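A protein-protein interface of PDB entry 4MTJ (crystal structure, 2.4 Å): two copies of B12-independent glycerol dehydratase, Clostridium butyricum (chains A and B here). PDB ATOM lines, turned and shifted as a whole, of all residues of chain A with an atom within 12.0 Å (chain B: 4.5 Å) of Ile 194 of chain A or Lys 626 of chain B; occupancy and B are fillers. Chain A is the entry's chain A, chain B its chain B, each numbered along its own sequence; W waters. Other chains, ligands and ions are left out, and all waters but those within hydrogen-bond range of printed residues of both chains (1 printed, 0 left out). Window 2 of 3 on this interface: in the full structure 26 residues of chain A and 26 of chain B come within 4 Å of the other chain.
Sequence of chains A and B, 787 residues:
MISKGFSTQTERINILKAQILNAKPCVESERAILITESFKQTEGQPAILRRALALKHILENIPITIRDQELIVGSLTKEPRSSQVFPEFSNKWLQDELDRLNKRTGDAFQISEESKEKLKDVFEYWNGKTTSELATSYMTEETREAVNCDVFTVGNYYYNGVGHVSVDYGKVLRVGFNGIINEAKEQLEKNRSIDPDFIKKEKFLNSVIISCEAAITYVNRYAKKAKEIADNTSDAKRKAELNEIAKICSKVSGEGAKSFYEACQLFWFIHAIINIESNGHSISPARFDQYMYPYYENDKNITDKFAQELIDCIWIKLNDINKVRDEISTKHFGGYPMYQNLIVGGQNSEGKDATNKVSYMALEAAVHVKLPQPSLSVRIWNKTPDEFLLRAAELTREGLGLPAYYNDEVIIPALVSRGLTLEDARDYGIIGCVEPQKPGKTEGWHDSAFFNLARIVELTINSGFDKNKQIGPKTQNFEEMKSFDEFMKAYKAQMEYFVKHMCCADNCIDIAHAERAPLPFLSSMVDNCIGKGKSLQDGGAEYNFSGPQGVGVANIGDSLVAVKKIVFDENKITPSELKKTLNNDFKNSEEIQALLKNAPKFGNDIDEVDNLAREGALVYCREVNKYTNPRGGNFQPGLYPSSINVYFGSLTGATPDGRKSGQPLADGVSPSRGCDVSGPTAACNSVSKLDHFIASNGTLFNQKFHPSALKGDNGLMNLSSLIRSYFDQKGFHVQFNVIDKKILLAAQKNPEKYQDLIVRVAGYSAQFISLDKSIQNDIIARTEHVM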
ATOM      1  N   GLN A 187      14.442  -1.878   9.507  1.00  0.00           N
ATOM      2  CA  GLN A 187      13.789  -2.933  10.280  1.00  0.00           C
ATOM      3  C   GLN A 187      12.608  -2.322  11.033  1.00  0.00           C
ATOM      4  O   GLN A 187      11.527  -2.905  11.105  1.00  0.00           O
ATOM      5  CB  GLN A 187      14.784  -3.603  11.236  1.00  0.00           C
ATOM      6  CG  GLN A 187      14.280  -4.875  11.908  1.00  0.00           C
ATOM      7  CD  GLN A 187      13.928  -5.979  10.924  1.00  0.00           C
ATOM      8  OE1 GLN A 187      14.728  -6.348  10.071  1.00  0.00           O
ATOM      9  NE2 GLN A 187      12.714  -6.504  11.036  1.00  0.00           N
ATOM     10  N   LEU A 188      12.832  -1.125  11.563  1.00  0.00           N
ATOM     11  CA  LEU A 188      11.790  -0.316  12.174  1.00  0.00           C
ATOM     12  C   LEU A 188      10.587  -0.157  11.230  1.00  0.00           C
ATOM     13  O   LEU A 188       9.431  -0.295  11.645  1.00  0.00           O
ATOM     14  CB  LEU A 188      12.384   1.047  12.524  1.00  0.00           C
ATOM     15  CG  LEU A 188      12.260   1.611  13.935  1.00  0.00           C
ATOM     16  CD1 LEU A 188      12.058   0.518  14.977  1.00  0.00           C
ATOM     17  CD2 LEU A 188      13.479   2.476  14.253  1.00  0.00           C
ATOM     18  N   GLU A 189      10.876   0.117   9.958  1.00  0.00           N
ATOM     19  CA  GLU A 189       9.856   0.211   8.921  1.00  0.00           C
ATOM     20  C   GLU A 189       9.130  -1.109   8.662  1.00  0.00           C
ATOM     21  O   GLU A 189       7.912  -1.130   8.518  1.00  0.00           O
ATOM     22  CB  GLU A 189      10.465   0.723   7.615  1.00  0.00           C
ATOM     23  CG  GLU A 189      10.542   2.223   7.539  1.00  0.00           C
ATOM     24  CD  GLU A 189       9.221   2.870   7.892  1.00  0.00           C
ATOM     25  OE1 GLU A 189       8.220   2.606   7.187  1.00  0.00           O
ATOM     26  OE2 GLU A 189       9.183   3.629   8.887  1.00  0.00           O
ATOM     27  N   LYS A 190       9.871  -2.208   8.590  1.00  0.00           N
ATOM     28  CA  LYS A 190       9.243  -3.511   8.368  1.00  0.00           C
ATOM     29  C   LYS A 190       8.349  -3.905   9.546  1.00  0.00           C
ATOM     30  O   LYS A 190       7.359  -4.615   9.378  1.00  0.00           O
ATOM     31  CB  LYS A 190      10.303  -4.585   8.131  1.00  0.00           C
ATOM     32  CG  LYS A 190      11.219  -4.277   6.968  1.00  0.00           C
ATOM     33  CD  LYS A 190      12.221  -5.391   6.744  1.00  0.00           C
ATOM     34  CE  LYS A 190      13.065  -5.128   5.502  1.00  0.00           C
ATOM     35  NZ  LYS A 190      14.040  -6.240   5.262  1.00  0.00           N
ATOM     36  N   ASN A 191       8.706  -3.417  10.730  1.00  0.00           N
ATOM     37  CA  ASN A 191       8.037  -3.771  11.967  1.00  0.00           C
ATOM     38  C   ASN A 191       6.814  -2.913  12.273  1.00  0.00           C
ATOM     39  O   ASN A 191       6.147  -3.134  13.280  1.00  0.00           O
ATOM     40  CB  ASN A 191       9.020  -3.696  13.141  1.00  0.00           C
ATOM     41  CG  ASN A 191      10.056  -4.821  13.124  1.00  0.00           C
ATOM     42  OD1 ASN A 191      10.050  -5.689  12.248  1.00  0.00           O
ATOM     43  ND2 ASN A 191      10.954  -4.803  14.104  1.00  0.00           N
ATOM     44  N   ARG A 192       6.532  -1.926  11.427  1.00  0.00           N
ATOM     45  CA  ARG A 192       5.303  -1.142  11.575  1.00  0.00           C
ATOM     46  C   ARG A 192       4.135  -2.100  11.727  1.00  0.00           C
ATOM     47  O   ARG A 192       3.841  -2.885  10.819  1.00  0.00           O
ATOM     48  CB  ARG A 192       5.057  -0.247  10.361  1.00  0.00           C
ATOM     49  CG  ARG A 192       5.708   1.121  10.430  1.00  0.00           C
ATOM     50  CD  ARG A 192       5.312   1.974   9.219  1.00  0.00           C
ATOM     51  NE  ARG A 192       5.885   3.316   9.285  1.00  0.00           N
ATOM     52  CZ  ARG A 192       5.229   4.399   9.698  1.00  0.00           C
ATOM     53  NH1 ARG A 192       3.958   4.308  10.080  1.00  0.00           N
ATOM     54  NH2 ARG A 192       5.841   5.578   9.724  1.00  0.00           N
ATOM     55  N   SER A 193       3.490  -2.051  12.885  1.00  0.00           N
ATOM     56  CA  SER A 193       2.474  -3.036  13.227  1.00  0.00           C
ATOM     57  C   SER A 193       1.744  -2.651  14.505  1.00  0.00           C
ATOM     58  O   SER A 193       2.294  -1.965  15.365  1.00  0.00           O
ATOM     59  CB  SER A 193       3.114  -4.416  13.393  1.00  0.00           C
ATOM     60  OG  SER A 193       2.219  -5.341  13.981  1.00  0.00           O
ATOM     61  N   ILE A 194       0.501  -3.099  14.620  1.00  0.00           N
ATOM     62  CA  ILE A 194      -0.290  -2.847  15.813  1.00  0.00           C
ATOM     63  C   ILE A 194      -0.063  -3.949  16.855  1.00  0.00           C
ATOM     64  O   ILE A 194      -0.522  -3.842  17.987  1.00  0.00           O
ATOM     65  CB  ILE A 194      -1.785  -2.742  15.471  1.00  0.00           C
ATOM     66  CG1 ILE A 194      -2.230  -3.981  14.685  1.00  0.00           C
ATOM     67  CG2 ILE A 194      -2.053  -1.471  14.670  1.00  0.00           C
ATOM     68  CD1 ILE A 194      -3.720  -4.175  14.652  1.00  0.00           C
ATOM     69  N   ASP A 195       0.647  -5.002  16.456  1.00  0.00           N
ATOM     70  CA  ASP A 195       1.054  -6.073  17.356  1.00  0.00           C
ATOM     71  C   ASP A 195       1.920  -5.516  18.506  1.00  0.00           C
ATOM     72  O   ASP A 195       2.939  -4.867  18.266  1.00  0.00           O
ATOM     73  CB  ASP A 195       1.835  -7.120  16.546  1.00  0.00           C
ATOM     74  CG  ASP A 195       2.092  -8.413  17.311  1.00  0.00           C
ATOM     75  OD1 ASP A 195       1.967  -8.436  18.553  1.00  0.00           O
ATOM     76  OD2 ASP A 195       2.437  -9.419  16.649  1.00  0.00           O
ATOM     77  N   PRO A 196       1.518  -5.778  19.762  1.00  0.00           N
ATOM     78  CA  PRO A 196       2.266  -5.235  20.909  1.00  0.00           C
ATOM     79  C   PRO A 196       3.711  -5.739  20.972  1.00  0.00           C
ATOM     80  O   PRO A 196       4.564  -5.079  21.582  1.00  0.00           O
ATOM     81  CB  PRO A 196       1.501  -5.750  22.130  1.00  0.00           C
ATOM     82  CG  PRO A 196       0.245  -6.341  21.628  1.00  0.00           C
ATOM     83  CD  PRO A 196       0.336  -6.565  20.161  1.00  0.00           C
ATOM     84  N   ASP A 197       3.981  -6.890  20.356  1.00  0.00           N
ATOM     85  CA  ASP A 197       5.331  -7.455  20.343  1.00  0.00           C
ATOM     86  C   ASP A 197       6.358  -6.486  19.775  1.00  0.00           C
ATOM     87  O   ASP A 197       7.543  -6.572  20.069  1.00  0.00           O
ATOM     88  CB  ASP A 197       5.375  -8.756  19.536  1.00  0.00           C
ATOM     89  CG  ASP A 197       5.143  -9.983  20.399  1.00  0.00           C
ATOM     90  OD1 ASP A 197       5.294  -9.879  21.639  1.00  0.00           O
ATOM     91  OD2 ASP A 197       4.814 -11.053  19.839  1.00  0.00           O
ATOM     92  N   PHE A 198       5.902  -5.554  18.958  1.00  0.00           N
ATOM     93  CA  PHE A 198       6.828  -4.659  18.303  1.00  0.00           C
ATOM     94  C   PHE A 198       7.193  -3.452  19.163  1.00  0.00           C
ATOM     95  O   PHE A 198       8.134  -2.726  18.842  1.00  0.00           O
ATOM     96  CB  PHE A 198       6.323  -4.275  16.903  1.00  0.00           C
ATOM     97  CG  PHE A 198       6.341  -5.433  15.914  1.00  0.00           C
ATOM     98  CD1 PHE A 198       5.161  -6.082  15.552  1.00  0.00           C
ATOM     99  CD2 PHE A 198       7.543  -5.883  15.366  1.00  0.00           C
ATOM    100  CE1 PHE A 198       5.170  -7.139  14.648  1.00  0.00           C
ATOM    101  CE2 PHE A 198       7.566  -6.946  14.468  1.00  0.00           C
ATOM    102  CZ  PHE A 198       6.374  -7.576  14.108  1.00  0.00           C
ATOM    103  N   ILE A 199       6.476  -3.259  20.269  1.00  0.00           N
ATOM    104  CA  ILE A 199       6.789  -2.161  21.192  1.00  0.00           C
ATOM    105  C   ILE A 199       8.222  -2.267  21.742  1.00  0.00           C
ATOM    106  O   ILE A 199       9.031  -1.354  21.577  1.00  0.00           O
ATOM    107  CB  ILE A 199       5.739  -2.043  22.332  1.00  0.00           C
ATOM    108  CG1 ILE A 199       4.422  -1.483  21.787  1.00  0.00           C
ATOM    109  CG2 ILE A 199       6.242  -1.159  23.479  1.00  0.00           C
ATOM    110  CD1 ILE A 199       3.214  -1.831  22.638  1.00  0.00           C
ATOM    111  N   LYS A 200       8.544  -3.389  22.369  1.00  0.00           N
ATOM    112  CA  LYS A 200       9.883  -3.576  22.906  1.00  0.00           C
ATOM    113  C   LYS A 200      10.950  -3.639  21.805  1.00  0.00           C
ATOM    114  O   LYS A 200      12.069  -3.187  22.011  1.00  0.00           O
ATOM    115  CB  LYS A 200       9.953  -4.826  23.785  1.00  0.00           C
ATOM    116  CG  LYS A 200       9.386  -4.671  25.194  1.00  0.00           C
ATOM    117  CD  LYS A 200       9.322  -6.044  25.868  1.00  0.00           C
ATOM    118  CE  LYS A 200       8.925  -5.983  27.328  1.00  0.00           C
ATOM    119  NZ  LYS A 200       8.331  -7.277  27.775  1.00  0.00           N
ATOM    120  N   LYS A 201      10.614  -4.210  20.649  1.00  0.00           N
ATOM    121  CA  LYS A 201      11.575  -4.296  19.543  1.00  0.00           C
ATOM    122  C   LYS A 201      11.913  -2.899  19.042  1.00  0.00           C
ATOM    123  O   LYS A 201      13.021  -2.638  18.585  1.00  0.00           O
ATOM    124  CB  LYS A 201      11.045  -5.156  18.392  1.00  0.00           C
ATOM    125  CG  LYS A 201      10.846  -6.641  18.743  1.00  0.00           C
ATOM    126  CD  LYS A 201      10.429  -7.443  17.496  1.00  0.00           C
ATOM    127  CE  LYS A 201       9.543  -8.638  17.842  1.00  0.00           C
ATOM    128  NZ  LYS A 201      10.289  -9.778  18.452  1.00  0.00           N
ATOM    129  N   GLU A 202      10.953  -1.996  19.158  1.00  0.00           N
ATOM    130  CA  GLU A 202      11.141  -0.631  18.703  1.00  0.00           C
ATOM    131  C   GLU A 202      12.149   0.085  19.601  1.00  0.00           C
ATOM    132  O   GLU A 202      13.039   0.781  19.116  1.00  0.00           O
ATOM    133  CB  GLU A 202       9.807   0.122  18.688  1.00  0.00           C
ATOM    134  CG  GLU A 202       9.830   1.364  17.811  1.00  0.00           C
ATOM    135  CD  GLU A 202       9.215   2.592  18.465  1.00  0.00           C
ATOM    136  OE1 GLU A 202       9.171   2.662  19.718  1.00  0.00           O
ATOM    137  OE2 GLU A 202       8.781   3.496  17.713  1.00  0.00           O
ATOM    138  N   GLU B 496     -10.352   5.078  12.900  1.00  0.00           N
ATOM    139  CA  GLU B 496      -9.209   4.164  12.819  1.00  0.00           C
ATOM    140  C   GLU B 496      -7.943   4.745  13.438  1.00  0.00           C
ATOM    141  O   GLU B 496      -7.239   4.065  14.202  1.00  0.00           O
ATOM    142  CB  GLU B 496      -8.913   3.743  11.376  1.00  0.00           C
ATOM    143  CG  GLU B 496      -7.483   3.203  11.174  1.00  0.00           C
ATOM    144  CD  GLU B 496      -7.351   2.328   9.942  1.00  0.00           C
ATOM    145  OE1 GLU B 496      -8.358   1.697   9.558  1.00  0.00           O
ATOM    146  OE2 GLU B 496      -6.249   2.272   9.351  1.00  0.00           O
ATOM    147  N   LYS B 500      -6.535   3.309  17.145  1.00  0.00           N
ATOM    148  CA  LYS B 500      -5.198   2.732  17.052  1.00  0.00           C
ATOM    149  C   LYS B 500      -4.282   3.270  18.142  1.00  0.00           C
ATOM    150  O   LYS B 500      -3.712   2.505  18.926  1.00  0.00           O
ATOM    151  CB  LYS B 500      -4.568   3.010  15.687  1.00  0.00           C
ATOM    152  CG  LYS B 500      -3.286   2.234  15.455  1.00  0.00           C
ATOM    153  CD  LYS B 500      -2.282   3.012  14.638  1.00  0.00           C
ATOM    154  CE  LYS B 500      -2.727   3.208  13.209  1.00  0.00           C
ATOM    155  NZ  LYS B 500      -1.768   4.091  12.487  1.00  0.00           N
ATOM    156  N   ARG B 622     -15.771  -1.967  15.668  1.00  0.00           N
ATOM    157  CA  ARG B 622     -15.031  -2.803  14.725  1.00  0.00           C
ATOM    158  C   ARG B 622     -13.550  -2.460  14.766  1.00  0.00           C
ATOM    159  O   ARG B 622     -12.698  -3.347  14.639  1.00  0.00           O
ATOM    160  CB  ARG B 622     -15.593  -2.699  13.305  1.00  0.00           C
ATOM    161  CG  ARG B 622     -16.997  -3.275  13.144  1.00  0.00           C
ATOM    162  CD  ARG B 622     -17.436  -3.121  11.705  1.00  0.00           C
ATOM    163  NE  ARG B 622     -18.879  -3.293  11.509  1.00  0.00           N
ATOM    164  CZ  ARG B 622     -19.690  -2.330  11.080  1.00  0.00           C
ATOM    165  NH1 ARG B 622     -19.207  -1.114  10.812  1.00  0.00           N
ATOM    166  NH2 ARG B 622     -20.981  -2.581  10.918  1.00  0.00           N
ATOM    167  N   GLU B 623     -13.255  -1.176  14.974  1.00  0.00           N
ATOM    168  CA  GLU B 623     -11.875  -0.715  15.145  1.00  0.00           C
ATOM    169  C   GLU B 623     -11.195  -1.338  16.377  1.00  0.00           C
ATOM    170  O   GLU B 623     -10.090  -1.889  16.282  1.00  0.00           O
ATOM    171  CB  GLU B 623     -11.825   0.814  15.235  1.00  0.00           C
ATOM    172  CG  GLU B 623     -12.163   1.522  13.941  1.00  0.00           C
ATOM    173  CD  GLU B 623     -11.373   0.978  12.752  1.00  0.00           C
ATOM    174  OE1 GLU B 623     -10.167   0.658  12.917  1.00  0.00           O
ATOM    175  OE2 GLU B 623     -11.968   0.857  11.650  1.00  0.00           O
ATOM    176  N   VAL B 624     -11.860  -1.242  17.527  1.00  0.00           N
ATOM    177  CA  VAL B 624     -11.366  -1.825  18.769  1.00  0.00           C
ATOM    178  C   VAL B 624     -11.082  -3.334  18.643  1.00  0.00           C
ATOM    179  O   VAL B 624     -10.060  -3.821  19.127  1.00  0.00           O
ATOM    180  CB  VAL B 624     -12.355  -1.574  19.929  1.00  0.00           C
ATOM    181  CG1 VAL B 624     -11.897  -2.286  21.194  1.00  0.00           C
ATOM    182  CG2 VAL B 624     -12.542  -0.060  20.176  1.00  0.00           C
ATOM    183  N   ASN B 625     -11.975  -4.071  17.991  1.00  0.00           N
ATOM    184  CA  ASN B 625     -11.779  -5.514  17.807  1.00  0.00           C
ATOM    185  C   ASN B 625     -10.462  -5.916  17.106  1.00  0.00           C
ATOM    186  O   ASN B 625     -10.052  -7.065  17.158  1.00  0.00           O
ATOM    187  CB  ASN B 625     -12.966  -6.120  17.051  1.00  0.00           C
ATOM    188  CG  ASN B 625     -14.133  -6.467  17.959  1.00  0.00           C
ATOM    189  OD1 ASN B 625     -14.039  -6.437  19.193  1.00  0.00           O
ATOM    190  ND2 ASN B 625     -15.245  -6.829  17.344  1.00  0.00           N
ATOM    191  N   LYS B 626      -9.810  -4.968  16.448  1.00  0.00           N
ATOM    192  CA  LYS B 626      -8.605  -5.274  15.679  1.00  0.00           C
ATOM    193  C   LYS B 626      -7.401  -5.540  16.568  1.00  0.00           C
ATOM    194  O   LYS B 626      -6.431  -6.149  16.130  1.00  0.00           O
ATOM    195  CB  LYS B 626      -8.265  -4.131  14.727  1.00  0.00           C
ATOM    196  CG  LYS B 626      -9.275  -3.915  13.630  1.00  0.00           C
ATOM    197  CD  LYS B 626      -8.845  -2.742  12.757  1.00  0.00           C
ATOM    198  CE  LYS B 626      -9.816  -2.529  11.610  1.00  0.00           C
ATOM    199  NZ  LYS B 626      -9.447  -1.337  10.820  1.00  0.00           N
ATOM    200  N   TYR B 627      -7.478  -5.104  17.818  1.00  0.00           N
ATOM    201  CA  TYR B 627      -6.294  -5.031  18.679  1.00  0.00           C
ATOM    202  C   TYR B 627      -6.147  -6.169  19.682  1.00  0.00           C
ATOM    203  O   TYR B 627      -7.135  -6.732  20.153  1.00  0.00           O
ATOM    204  CB  TYR B 627      -6.236  -3.657  19.364  1.00  0.00           C
ATOM    205  CG  TYR B 627      -6.121  -2.587  18.326  1.00  0.00           C
ATOM    206  CD1 TYR B 627      -7.255  -2.074  17.700  1.00  0.00           C
ATOM    207  CD2 TYR B 627      -4.877  -2.142  17.902  1.00  0.00           C
ATOM    208  CE1 TYR B 627      -7.155  -1.120  16.713  1.00  0.00           C
ATOM    209  CE2 TYR B 627      -4.761  -1.184  16.917  1.00  0.00           C
ATOM    210  CZ  TYR B 627      -5.901  -0.680  16.328  1.00  0.00           C
ATOM    211  OH  TYR B 627      -5.788   0.257  15.341  1.00  0.00           O
ATOM    212  N   THR B 628      -4.898  -6.515  19.975  1.00  0.00           N
ATOM    213  CA  THR B 628      -4.598  -7.477  21.014  1.00  0.00           C
ATOM    214  C   THR B 628      -3.619  -6.852  22.019  1.00  0.00           C
ATOM    215  O   THR B 628      -2.913  -5.906  21.696  1.00  0.00           O
ATOM    216  CB  THR B 628      -4.023  -8.783  20.435  1.00  0.00           C
ATOM    217  OG1 THR B 628      -2.672  -8.568  20.036  1.00  0.00           O
ATOM    218  CG2 THR B 628      -4.824  -9.251  19.231  1.00  0.00           C
HETATM  219  O   HOH W   1      -2.954  -5.273  18.169  1.00  0.00           O
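OE1 of Glu 496 of chain B lies within salt-bridge range of NZ of Lys 626 of chain B, 3.5 Å away.
The side-chain carboxylate (OE1) of Glu 623 of chain B lies within salt-bridge range of the side-chain amino group (NZ) of Lys 626 of chain B (3.0 Å).
Printed residues of chain B within 4 Å of Ile 194 of chain A: Lys 500, Lys 626 and Tyr 627.
Of the printed residues of chain A, Lys 626 of chain B touches Ile 194 (3.7 Å).
No residue of chain A comes within 4 Å of Val 624 of chain B.
No residue of chain A comes within 4 Å of Asn 625 of chain B.
Of the printed residues of chain B, Pro 196 of chain A touches Thr 628 (3.2 Å).
Of the printed residues of chain A, Lys 500 of chain B touches Ile 194 (3.98 Å).
Ile 199 of chain A touches none of the printed residues of chain B.
The nearest printed residue of chain B that does not touch Ile 194 of chain A is Thr 628 of chain B (4.9 Å).
Of the 9 printed residues of chain B, 4 touch a printed residue of chain A.
Hydrophobic or aromatic side chains of chain B that line the printed part of chain A: Tyr 627.
Among the printed residues, 4 pairs touch across the chains.
Among the printed residues, no Asp or Glu carboxylate lies within 4 Å of a Lys or Arg side-chain nitrogen of the other chain.
No position is printed for both chains.
Of the 4 pairs that touch across the chains among the printed residues, none has its exchanged pair printed and touching as well.
Among the printed residues, merely in contact across the chains: Ile 194 of chain A with Lys 500 of chain B (3.98 Å), Ile 194 of chain A with Lys 626 of chain B (3.7 Å), Ile 194 of chain A with Tyr 627 of chain B (3.5 Å) and Pro 196 of chain A with Thr 628 of chain B (3.2 Å).
Water W1 lies within hydrogen-bond range of the backbone carbonyl oxygen of Ile 194 of chain A and the backbone NH of Thr 628 of chain B.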
